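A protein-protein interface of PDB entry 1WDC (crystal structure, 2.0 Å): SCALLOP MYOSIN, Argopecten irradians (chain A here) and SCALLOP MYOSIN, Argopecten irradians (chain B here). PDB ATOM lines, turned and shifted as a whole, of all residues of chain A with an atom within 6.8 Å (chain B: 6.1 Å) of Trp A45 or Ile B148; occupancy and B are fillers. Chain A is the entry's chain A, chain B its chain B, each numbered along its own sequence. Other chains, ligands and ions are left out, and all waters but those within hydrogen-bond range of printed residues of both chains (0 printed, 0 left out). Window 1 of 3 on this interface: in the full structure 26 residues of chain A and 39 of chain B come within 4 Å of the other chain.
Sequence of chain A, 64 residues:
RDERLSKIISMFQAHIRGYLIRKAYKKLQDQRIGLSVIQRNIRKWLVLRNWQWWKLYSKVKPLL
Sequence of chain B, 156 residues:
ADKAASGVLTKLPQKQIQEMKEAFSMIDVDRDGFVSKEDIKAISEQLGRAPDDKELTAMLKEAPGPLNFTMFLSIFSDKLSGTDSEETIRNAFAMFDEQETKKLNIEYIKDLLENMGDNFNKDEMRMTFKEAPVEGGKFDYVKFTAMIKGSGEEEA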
ATOM      1  N   ILE A  38       2.525   4.770 -18.081  1.00  0.00           N
ATOM      2  CA  ILE A  38       3.073   5.543 -19.193  1.00  0.00           C
ATOM      3  C   ILE A  38       2.975   4.708 -20.465  1.00  0.00           C
ATOM      4  O   ILE A  38       2.547   5.214 -21.482  1.00  0.00           O
ATOM      5  CB  ILE A  38       4.613   5.933 -18.933  1.00  0.00           C
ATOM      6  CG1 ILE A  38       4.734   7.004 -17.826  1.00  0.00           C
ATOM      7  CG2 ILE A  38       5.269   6.440 -20.194  1.00  0.00           C
ATOM      8  CD1 ILE A  38       6.142   7.054 -17.188  1.00  0.00           C
ATOM      9  N   ARG A  40       0.969   2.070 -21.155  1.00  0.00           N
ATOM     10  CA  ARG A  40      -0.366   1.697 -21.590  1.00  0.00           C
ATOM     11  C   ARG A  40      -1.196   2.868 -22.103  1.00  0.00           C
ATOM     12  O   ARG A  40      -1.958   2.731 -23.079  1.00  0.00           O
ATOM     13  CB  ARG A  40      -1.108   0.959 -20.481  1.00  0.00           C
ATOM     14  CG  ARG A  40      -1.656   1.829 -19.404  1.00  0.00           C
ATOM     15  CD  ARG A  40      -2.723   1.098 -18.656  1.00  0.00           C
ATOM     16  NE  ARG A  40      -3.127   1.863 -17.493  1.00  0.00           N
ATOM     17  CZ  ARG A  40      -2.583   1.716 -16.296  1.00  0.00           C
ATOM     18  NH1 ARG A  40      -1.595   0.846 -16.109  1.00  0.00           N
ATOM     19  NH2 ARG A  40      -3.066   2.403 -15.267  1.00  0.00           N
ATOM     20  N   ASN A  41      -0.892   4.047 -21.580  1.00  0.00           N
ATOM     21  CA  ASN A  41      -1.557   5.267 -22.000  1.00  0.00           C
ATOM     22  C   ASN A  41      -1.010   5.911 -23.293  1.00  0.00           C
ATOM     23  O   ASN A  41      -1.760   6.522 -24.043  1.00  0.00           O
ATOM     24  CB  ASN A  41      -1.540   6.273 -20.859  1.00  0.00           C
ATOM     25  CG  ASN A  41      -2.671   6.055 -19.866  1.00  0.00           C
ATOM     26  OD1 ASN A  41      -3.766   6.557 -20.076  1.00  0.00           O
ATOM     27  ND2 ASN A  41      -2.375   5.428 -18.722  1.00  0.00           N
ATOM     28  N   ILE A  42       0.288   5.805 -23.540  1.00  0.00           N
ATOM     29  CA  ILE A  42       0.853   6.184 -24.830  1.00  0.00           C
ATOM     30  C   ILE A  42       0.236   5.333 -25.945  1.00  0.00           C
ATOM     31  O   ILE A  42      -0.127   5.840 -26.997  1.00  0.00           O
ATOM     32  CB  ILE A  42       2.413   6.021 -24.839  1.00  0.00           C
ATOM     33  CG1 ILE A  42       3.029   7.071 -23.880  1.00  0.00           C
ATOM     34  CG2 ILE A  42       2.979   6.159 -26.289  1.00  0.00           C
ATOM     35  CD1 ILE A  42       4.545   7.014 -23.776  1.00  0.00           C
ATOM     36  N   ARG A  43       0.073   4.054 -25.663  1.00  0.00           N
ATOM     37  CA  ARG A  43      -0.542   3.112 -26.593  1.00  0.00           C
ATOM     38  C   ARG A  43      -2.041   3.299 -26.909  1.00  0.00           C
ATOM     39  O   ARG A  43      -2.472   2.911 -27.962  1.00  0.00           O
ATOM     40  CB  ARG A  43      -0.316   1.700 -26.083  1.00  0.00           C
ATOM     41  CG  ARG A  43       1.079   1.194 -26.347  1.00  0.00           C
ATOM     42  CD  ARG A  43       1.223  -0.157 -25.729  1.00  0.00           C
ATOM     43  NE  ARG A  43       2.314  -0.894 -26.316  1.00  0.00           N
ATOM     44  CZ  ARG A  43       3.272  -1.448 -25.602  1.00  0.00           C
ATOM     45  NH1 ARG A  43       3.207  -1.405 -24.274  1.00  0.00           N
ATOM     46  NH2 ARG A  43       4.276  -2.035 -26.218  1.00  0.00           N
ATOM     47  N   LYS A  44      -2.832   3.660 -25.913  1.00  0.00           N
ATOM     48  CA  LYS A  44      -4.182   4.155 -26.120  1.00  0.00           C
ATOM     49  C   LYS A  44      -4.194   5.325 -27.058  1.00  0.00           C
ATOM     50  O   LYS A  44      -5.118   5.464 -27.853  1.00  0.00           O
ATOM     51  CB  LYS A  44      -4.806   4.589 -24.810  1.00  0.00           C
ATOM     52  CG  LYS A  44      -5.142   3.424 -23.894  1.00  0.00           C
ATOM     53  CD  LYS A  44      -6.630   3.295 -23.664  1.00  0.00           C
ATOM     54  CE  LYS A  44      -7.069   1.842 -23.876  1.00  0.00           C
ATOM     55  NZ  LYS A  44      -7.882   1.333 -22.720  1.00  0.00           N
ATOM     56  N   TRP A  45      -3.193   6.191 -26.933  1.00  0.00           N
ATOM     57  CA  TRP A  45      -3.059   7.363 -27.786  1.00  0.00           C
ATOM     58  C   TRP A  45      -2.749   6.940 -29.207  1.00  0.00           C
ATOM     59  O   TRP A  45      -3.454   7.287 -30.146  1.00  0.00           O
ATOM     60  CB  TRP A  45      -1.942   8.251 -27.270  1.00  0.00           C
ATOM     61  CG  TRP A  45      -1.665   9.442 -28.095  1.00  0.00           C
ATOM     62  CD1 TRP A  45      -2.478  10.528 -28.273  1.00  0.00           C
ATOM     63  CD2 TRP A  45      -0.420   9.760 -28.732  1.00  0.00           C
ATOM     64  NE1 TRP A  45      -1.796  11.516 -28.957  1.00  0.00           N
ATOM     65  CE2 TRP A  45      -0.536  11.070 -29.254  1.00  0.00           C
ATOM     66  CE3 TRP A  45       0.784   9.063 -28.912  1.00  0.00           C
ATOM     67  CZ2 TRP A  45       0.503  11.696 -29.943  1.00  0.00           C
ATOM     68  CZ3 TRP A  45       1.821   9.689 -29.624  1.00  0.00           C
ATOM     69  CH2 TRP A  45       1.669  10.989 -30.127  1.00  0.00           C
ATOM     70  N   LEU A  46      -1.786   6.060 -29.353  1.00  0.00           N
ATOM     71  CA  LEU A  46      -1.480   5.555 -30.668  1.00  0.00           C
ATOM     72  C   LEU A  46      -2.686   4.913 -31.337  1.00  0.00           C
ATOM     73  O   LEU A  46      -2.894   5.116 -32.493  1.00  0.00           O
ATOM     74  CB  LEU A  46      -0.343   4.556 -30.577  1.00  0.00           C
ATOM     75  CG  LEU A  46       0.962   5.144 -30.031  1.00  0.00           C
ATOM     76  CD1 LEU A  46       1.991   4.032 -29.740  1.00  0.00           C
ATOM     77  CD2 LEU A  46       1.464   6.100 -31.042  1.00  0.00           C
ATOM     78  N   VAL A  47      -3.476   4.151 -30.595  1.00  0.00           N
ATOM     79  CA  VAL A  47      -4.696   3.533 -31.115  1.00  0.00           C
ATOM     80  C   VAL A  47      -5.698   4.606 -31.512  1.00  0.00           C
ATOM     81  O   VAL A  47      -6.257   4.566 -32.614  1.00  0.00           O
ATOM     82  CB  VAL A  47      -5.360   2.567 -30.071  1.00  0.00           C
ATOM     83  CG1 VAL A  47      -6.867   2.529 -30.230  1.00  0.00           C
ATOM     84  CG2 VAL A  47      -4.819   1.171 -30.228  1.00  0.00           C
ATOM     85  N   LEU A  48      -5.862   5.600 -30.652  1.00  0.00           N
ATOM     86  CA  LEU A  48      -6.797   6.659 -30.941  1.00  0.00           C
ATOM     87  C   LEU A  48      -6.375   7.423 -32.195  1.00  0.00           C
ATOM     88  O   LEU A  48      -7.213   7.735 -33.052  1.00  0.00           O
ATOM     89  CB  LEU A  48      -6.930   7.587 -29.744  1.00  0.00           C
ATOM     90  CG  LEU A  48      -8.055   8.622 -29.784  1.00  0.00           C
ATOM     91  CD1 LEU A  48      -9.422   7.995 -29.942  1.00  0.00           C
ATOM     92  CD2 LEU A  48      -8.022   9.380 -28.514  1.00  0.00           C
ATOM     93  N   ARG A  49      -5.072   7.508 -32.426  1.00  0.00           N
ATOM     94  CA  ARG A  49      -4.550   8.355 -33.508  1.00  0.00           C
ATOM     95  C   ARG A  49      -4.802   7.762 -34.912  1.00  0.00           C
ATOM     96  O   ARG A  49      -4.681   8.447 -35.921  1.00  0.00           O
ATOM     97  CB  ARG A  49      -3.046   8.603 -33.294  1.00  0.00           C
ATOM     98  CG  ARG A  49      -2.717   9.891 -32.558  1.00  0.00           C
ATOM     99  CD  ARG A  49      -1.363  10.488 -33.019  1.00  0.00           C
ATOM    100  NE  ARG A  49      -1.505  11.803 -33.668  1.00  0.00           N
ATOM    101  CZ  ARG A  49      -1.892  12.936 -33.064  1.00  0.00           C
ATOM    102  NH1 ARG A  49      -2.135  12.988 -31.754  1.00  0.00           N
ATOM    103  NH2 ARG A  49      -2.037  14.044 -33.781  1.00  0.00           N
ATOM    104  N   ASN A  50      -5.140   6.479 -34.944  1.00  0.00           N
ATOM    105  CA  ASN A  50      -5.428   5.778 -36.181  1.00  0.00           C
ATOM    106  C   ASN A  50      -6.876   5.319 -36.295  1.00  0.00           C
ATOM    107  O   ASN A  50      -7.248   4.581 -37.203  1.00  0.00           O
ATOM    108  CB  ASN A  50      -4.504   4.576 -36.334  1.00  0.00           C
ATOM    109  CG  ASN A  50      -3.503   4.769 -37.461  1.00  0.00           C
ATOM    110  OD1 ASN A  50      -2.613   5.641 -37.361  1.00  0.00           O
ATOM    111  ND2 ASN A  50      -3.729   4.076 -38.602  1.00  0.00           N
ATOM    112  N   TRP A  54     -11.704   9.514 -34.925  1.00  0.00           N
ATOM    113  CA  TRP A  54     -10.765  10.485 -34.345  1.00  0.00           C
ATOM    114  C   TRP A  54     -10.137  11.338 -35.421  1.00  0.00           C
ATOM    115  O   TRP A  54     -10.116  12.568 -35.295  1.00  0.00           O
ATOM    116  CB  TRP A  54      -9.638   9.781 -33.582  1.00  0.00           C
ATOM    117  CG  TRP A  54      -8.915  10.738 -32.666  1.00  0.00           C
ATOM    118  CD1 TRP A  54      -7.648  11.277 -32.850  1.00  0.00           C
ATOM    119  CD2 TRP A  54      -9.528  11.516 -31.623  1.00  0.00           C
ATOM    120  NE1 TRP A  54      -7.480  12.377 -32.029  1.00  0.00           N
ATOM    121  CE2 TRP A  54      -8.623  12.556 -31.283  1.00  0.00           C
ATOM    122  CE3 TRP A  54     -10.778  11.463 -30.977  1.00  0.00           C
ATOM    123  CZ2 TRP A  54      -8.944  13.540 -30.346  1.00  0.00           C
ATOM    124  CZ3 TRP A  54     -11.098  12.441 -30.039  1.00  0.00           C
ATOM    125  CH2 TRP A  54     -10.187  13.468 -29.737  1.00  0.00           C
ATOM    126  N   ILE B  89      -1.019  10.418 -15.215  1.00  0.00           N
ATOM    127  CA  ILE B  89       0.022  10.238 -16.228  1.00  0.00           C
ATOM    128  C   ILE B  89       1.230  11.147 -15.979  1.00  0.00           C
ATOM    129  O   ILE B  89       2.362  10.695 -16.034  1.00  0.00           O
ATOM    130  CB  ILE B  89      -0.518  10.494 -17.675  1.00  0.00           C
ATOM    131  CG1 ILE B  89      -1.760   9.623 -17.964  1.00  0.00           C
ATOM    132  CG2 ILE B  89       0.594  10.186 -18.715  1.00  0.00           C
ATOM    133  CD1 ILE B  89      -2.519  10.000 -19.251  1.00  0.00           C
ATOM    134  N   MET B 127       6.654   6.135 -33.654  1.00  0.00           N
ATOM    135  CA  MET B 127       5.399   6.899 -33.639  1.00  0.00           C
ATOM    136  C   MET B 127       5.250   7.804 -32.434  1.00  0.00           C
ATOM    137  O   MET B 127       4.636   8.855 -32.521  1.00  0.00           O
ATOM    138  CB  MET B 127       4.181   5.967 -33.704  1.00  0.00           C
ATOM    139  CG  MET B 127       3.870   5.371 -35.086  1.00  0.00           C
ATOM    140  SD  MET B 127       4.299   6.462 -36.522  1.00  0.00           S
ATOM    141  CE  MET B 127       3.257   7.964 -36.228  1.00  0.00           C
ATOM    142  N   THR B 128       5.746   7.357 -31.290  1.00  0.00           N
ATOM    143  CA  THR B 128       5.651   8.139 -30.073  1.00  0.00           C
ATOM    144  C   THR B 128       6.472   9.389 -30.192  1.00  0.00           C
ATOM    145  O   THR B 128       6.024  10.478 -29.838  1.00  0.00           O
ATOM    146  CB  THR B 128       6.180   7.340 -28.929  1.00  0.00           C
ATOM    147  OG1 THR B 128       5.341   6.209 -28.752  1.00  0.00           O
ATOM    148  CG2 THR B 128       6.192   8.144 -27.678  1.00  0.00           C
ATOM    149  N   PHE B 129       7.694   9.219 -30.683  1.00  0.00           N
ATOM    150  CA  PHE B 129       8.657  10.310 -30.665  1.00  0.00           C
ATOM    151  C   PHE B 129       8.646  11.163 -31.953  1.00  0.00           C
ATOM    152  O   PHE B 129       9.201  12.261 -31.972  1.00  0.00           O
ATOM    153  CB  PHE B 129      10.078   9.778 -30.368  1.00  0.00           C
ATOM    154  CG  PHE B 129      10.271   9.290 -28.948  1.00  0.00           C
ATOM    155  CD1 PHE B 129      10.351  10.179 -27.895  1.00  0.00           C
ATOM    156  CD2 PHE B 129      10.224   7.938 -28.652  1.00  0.00           C
ATOM    157  CE1 PHE B 129      10.353   9.709 -26.568  1.00  0.00           C
ATOM    158  CE2 PHE B 129      10.222   7.490 -27.330  1.00  0.00           C
ATOM    159  CZ  PHE B 129      10.279   8.369 -26.313  1.00  0.00           C
ATOM    160  N   GLU B 131       6.107  12.686 -32.531  1.00  0.00           N
ATOM    161  CA  GLU B 131       5.222  13.741 -32.072  1.00  0.00           C
ATOM    162  C   GLU B 131       5.737  14.546 -30.863  1.00  0.00           C
ATOM    163  O   GLU B 131       5.372  15.717 -30.695  1.00  0.00           O
ATOM    164  CB  GLU B 131       3.856  13.131 -31.776  1.00  0.00           C
ATOM    165  CG  GLU B 131       2.702  13.805 -32.527  1.00  0.00           C
ATOM    166  CD  GLU B 131       2.954  13.957 -34.033  1.00  0.00           C
ATOM    167  OE1 GLU B 131       3.379  12.971 -34.685  1.00  0.00           O
ATOM    168  OE2 GLU B 131       2.696  15.061 -34.570  1.00  0.00           O
ATOM    169  N   ALA B 132       6.759  13.994 -30.206  1.00  0.00           N
ATOM    170  CA  ALA B 132       7.180  14.384 -28.856  1.00  0.00           C
ATOM    171  C   ALA B 132       7.876  15.759 -28.762  1.00  0.00           C
ATOM    172  O   ALA B 132       8.727  16.105 -29.597  1.00  0.00           O
ATOM    173  CB  ALA B 132       8.083  13.304 -28.279  1.00  0.00           C
ATOM    174  N   LYS B 143       4.224  18.466 -21.229  1.00  0.00           N
ATOM    175  CA  LYS B 143       3.565  18.891 -22.448  1.00  0.00           C
ATOM    176  C   LYS B 143       3.106  17.721 -23.217  1.00  0.00           C
ATOM    177  O   LYS B 143       2.137  17.818 -23.937  1.00  0.00           O
ATOM    178  CB  LYS B 143       4.488  19.704 -23.342  1.00  0.00           C
ATOM    179  CG  LYS B 143       4.101  21.175 -23.411  1.00  0.00           C
ATOM    180  CD  LYS B 143       2.607  21.404 -22.990  1.00  0.00           C
ATOM    181  CE  LYS B 143       2.460  21.800 -21.494  1.00  0.00           C
ATOM    182  NZ  LYS B 143       1.093  21.517 -20.901  1.00  0.00           N
ATOM    183  N   PHE B 144       3.951  16.707 -23.261  1.00  0.00           N
ATOM    184  CA  PHE B 144       3.585  15.451 -23.876  1.00  0.00           C
ATOM    185  C   PHE B 144       2.298  14.854 -23.253  1.00  0.00           C
ATOM    186  O   PHE B 144       1.463  14.288 -23.956  1.00  0.00           O
ATOM    187  CB  PHE B 144       4.735  14.467 -23.740  1.00  0.00           C
ATOM    188  CG  PHE B 144       4.435  13.119 -24.319  1.00  0.00           C
ATOM    189  CD1 PHE B 144       4.592  12.884 -25.675  1.00  0.00           C
ATOM    190  CD2 PHE B 144       4.013  12.070 -23.501  1.00  0.00           C
ATOM    191  CE1 PHE B 144       4.344  11.615 -26.204  1.00  0.00           C
ATOM    192  CE2 PHE B 144       3.767  10.816 -24.026  1.00  0.00           C
ATOM    193  CZ  PHE B 144       3.932  10.586 -25.372  1.00  0.00           C
ATOM    194  N   THR B 145       2.165  14.921 -21.935  1.00  0.00           N
ATOM    195  CA  THR B 145       0.964  14.418 -21.284  1.00  0.00           C
ATOM    196  C   THR B 145      -0.293  15.174 -21.729  1.00  0.00           C
ATOM    197  O   THR B 145      -1.282  14.538 -22.085  1.00  0.00           O
ATOM    198  CB  THR B 145       1.105  14.481 -19.755  1.00  0.00           C
ATOM    199  OG1 THR B 145       2.222  13.675 -19.343  1.00  0.00           O
ATOM    200  CG2 THR B 145      -0.150  13.980 -19.090  1.00  0.00           C
ATOM    201  N   ALA B 146      -0.253  16.511 -21.726  1.00  0.00           N
ATOM    202  CA  ALA B 146      -1.311  17.328 -22.312  1.00  0.00           C
ATOM    203  C   ALA B 146      -1.654  16.932 -23.768  1.00  0.00           C
ATOM    204  O   ALA B 146      -2.799  16.634 -24.071  1.00  0.00           O
ATOM    205  CB  ALA B 146      -0.924  18.780 -22.238  1.00  0.00           C
ATOM    206  N   MET B 147      -0.634  16.795 -24.612  1.00  0.00           N
ATOM    207  CA  MET B 147      -0.772  16.304 -25.978  1.00  0.00           C
ATOM    208  C   MET B 147      -1.453  14.952 -26.047  1.00  0.00           C
ATOM    209  O   MET B 147      -2.208  14.683 -26.973  1.00  0.00           O
ATOM    210  CB  MET B 147       0.601  16.186 -26.645  1.00  0.00           C
ATOM    211  CG  MET B 147       0.678  15.122 -27.739  1.00  0.00           C
ATOM    212  SD  MET B 147       2.047  15.362 -28.917  1.00  0.00           S
ATOM    213  CE  MET B 147       2.842  13.806 -28.781  1.00  0.00           C
ATOM    214  N   ILE B 148      -1.032  14.045 -25.176  1.00  0.00           N
ATOM    215  CA  ILE B 148      -1.575  12.687 -25.105  1.00  0.00           C
ATOM    216  C   ILE B 148      -2.997  12.617 -24.504  1.00  0.00           C
ATOM    217  O   ILE B 148      -3.748  11.691 -24.797  1.00  0.00           O
ATOM    218  CB  ILE B 148      -0.582  11.791 -24.345  1.00  0.00           C
ATOM    219  CG1 ILE B 148       0.143  10.924 -25.336  1.00  0.00           C
ATOM    220  CG2 ILE B 148      -1.235  10.941 -23.255  1.00  0.00           C
ATOM    221  CD1 ILE B 148       0.545   9.628 -24.706  1.00  0.00           C
ATOM    222  N   LYS B 149      -3.415  13.686 -23.825  1.00  0.00           N
ATOM    223  CA  LYS B 149      -4.738  13.758 -23.233  1.00  0.00           C
ATOM    224  C   LYS B 149      -5.612  14.845 -23.830  1.00  0.00           C
ATOM    225  O   LYS B 149      -6.748  15.009 -23.406  1.00  0.00           O
ATOM    226  CB  LYS B 149      -4.630  13.979 -21.737  1.00  0.00           C
ATOM    227  CG  LYS B 149      -4.043  12.807 -21.016  1.00  0.00           C
ATOM    228  CD  LYS B 149      -5.086  12.158 -20.163  1.00  0.00           C
ATOM    229  CE  LYS B 149      -6.100  11.363 -20.991  1.00  0.00           C
ATOM    230  NZ  LYS B 149      -7.399  11.100 -20.253  1.00  0.00           N
ATOM    231  N   GLY B 150      -5.051  15.649 -24.732  1.00  0.00           N
ATOM    232  CA  GLY B 150      -5.825  16.675 -25.420  1.00  0.00           C
ATOM    233  C   GLY B 150      -5.936  18.040 -24.758  1.00  0.00           C
ATOM    234  O   GLY B 150      -6.512  18.960 -25.332  1.00  0.00           O
ATOM    235  N   GLU B 153      -3.176  18.614 -27.113  1.00  0.00           N
ATOM    236  CA  GLU B 153      -3.302  18.131 -28.485  1.00  0.00           C
ATOM    237  C   GLU B 153      -4.011  16.771 -28.629  1.00  0.00           C
ATOM    238  O   GLU B 153      -5.228  16.717 -28.337  1.00  0.00           O
ATOM    239  CB  GLU B 153      -1.913  18.095 -29.146  1.00  0.00           C
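OD1 of Asn A41 touches CD1 of Ile B89, at 3.8 Å. Ile B148 touches Asn A41 (CD1 to O, 3.9 Å). Ile A42 touches Thr B128. CG1 of Ile A42 touches CE2 of Phe B144 (3.8 Å). Ile A42 touches Ile B148 (CA to CD1, 3.5 Å). Trp A45 touches Glu B131 (CH2 to CB, 3.5 Å). CH2 of Trp A45 touches CE of Met B147 (3.3 Å). CG1 of Ile B148 touches CG of Trp A45, at 3.6 Å. Met B127 touches Leu A46 (CB to CD2, 3.8 Å).
Of the 13 printed residues of chain A, 4 touch a printed residue of chain B. Printed residues of chain B that touch a printed residue of chain A: Ile B89, Met B127, Thr B128, Glu B131, Phe B144, Met B147 and Ile B148. Hydrophobic or aromatic side chains of chain B that line the printed part of chain A: Ile B89, Met B127, Phe B144, Met B147 and Ile B148. Among the printed residues, no Asp or Glu carboxylate lies within 4 Å of a Lys or Arg side-chain nitrogen of the other chain.
Ile A38 touches none of the printed residues of chain B. Of chain B, only Glu B131 (3.5 Å), Met B147 (3.3 Å) and Ile B148 (3.6 Å) come within 4 Å of Trp A45. Of the printed residues of chain A, Met B127 touches Leu A46 (3.8 Å). Of the printed residues of chain A, Glu B131 touches Trp A45 (3.5 Å). Of the printed residues of chain A, Met B147 touches Trp A45. Ile B148 touches just these residues of chain A: Asn A41 (3.9 Å), Ile A42 (3.5 Å) and Trp A45 (3.6 Å). The nearest residue of chain A that does not touch Ile B148 is Arg A43 (5.7 Å). The nearest printed residue of chain A that does not touch Glu B131 is Arg A49 (4.7 Å).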
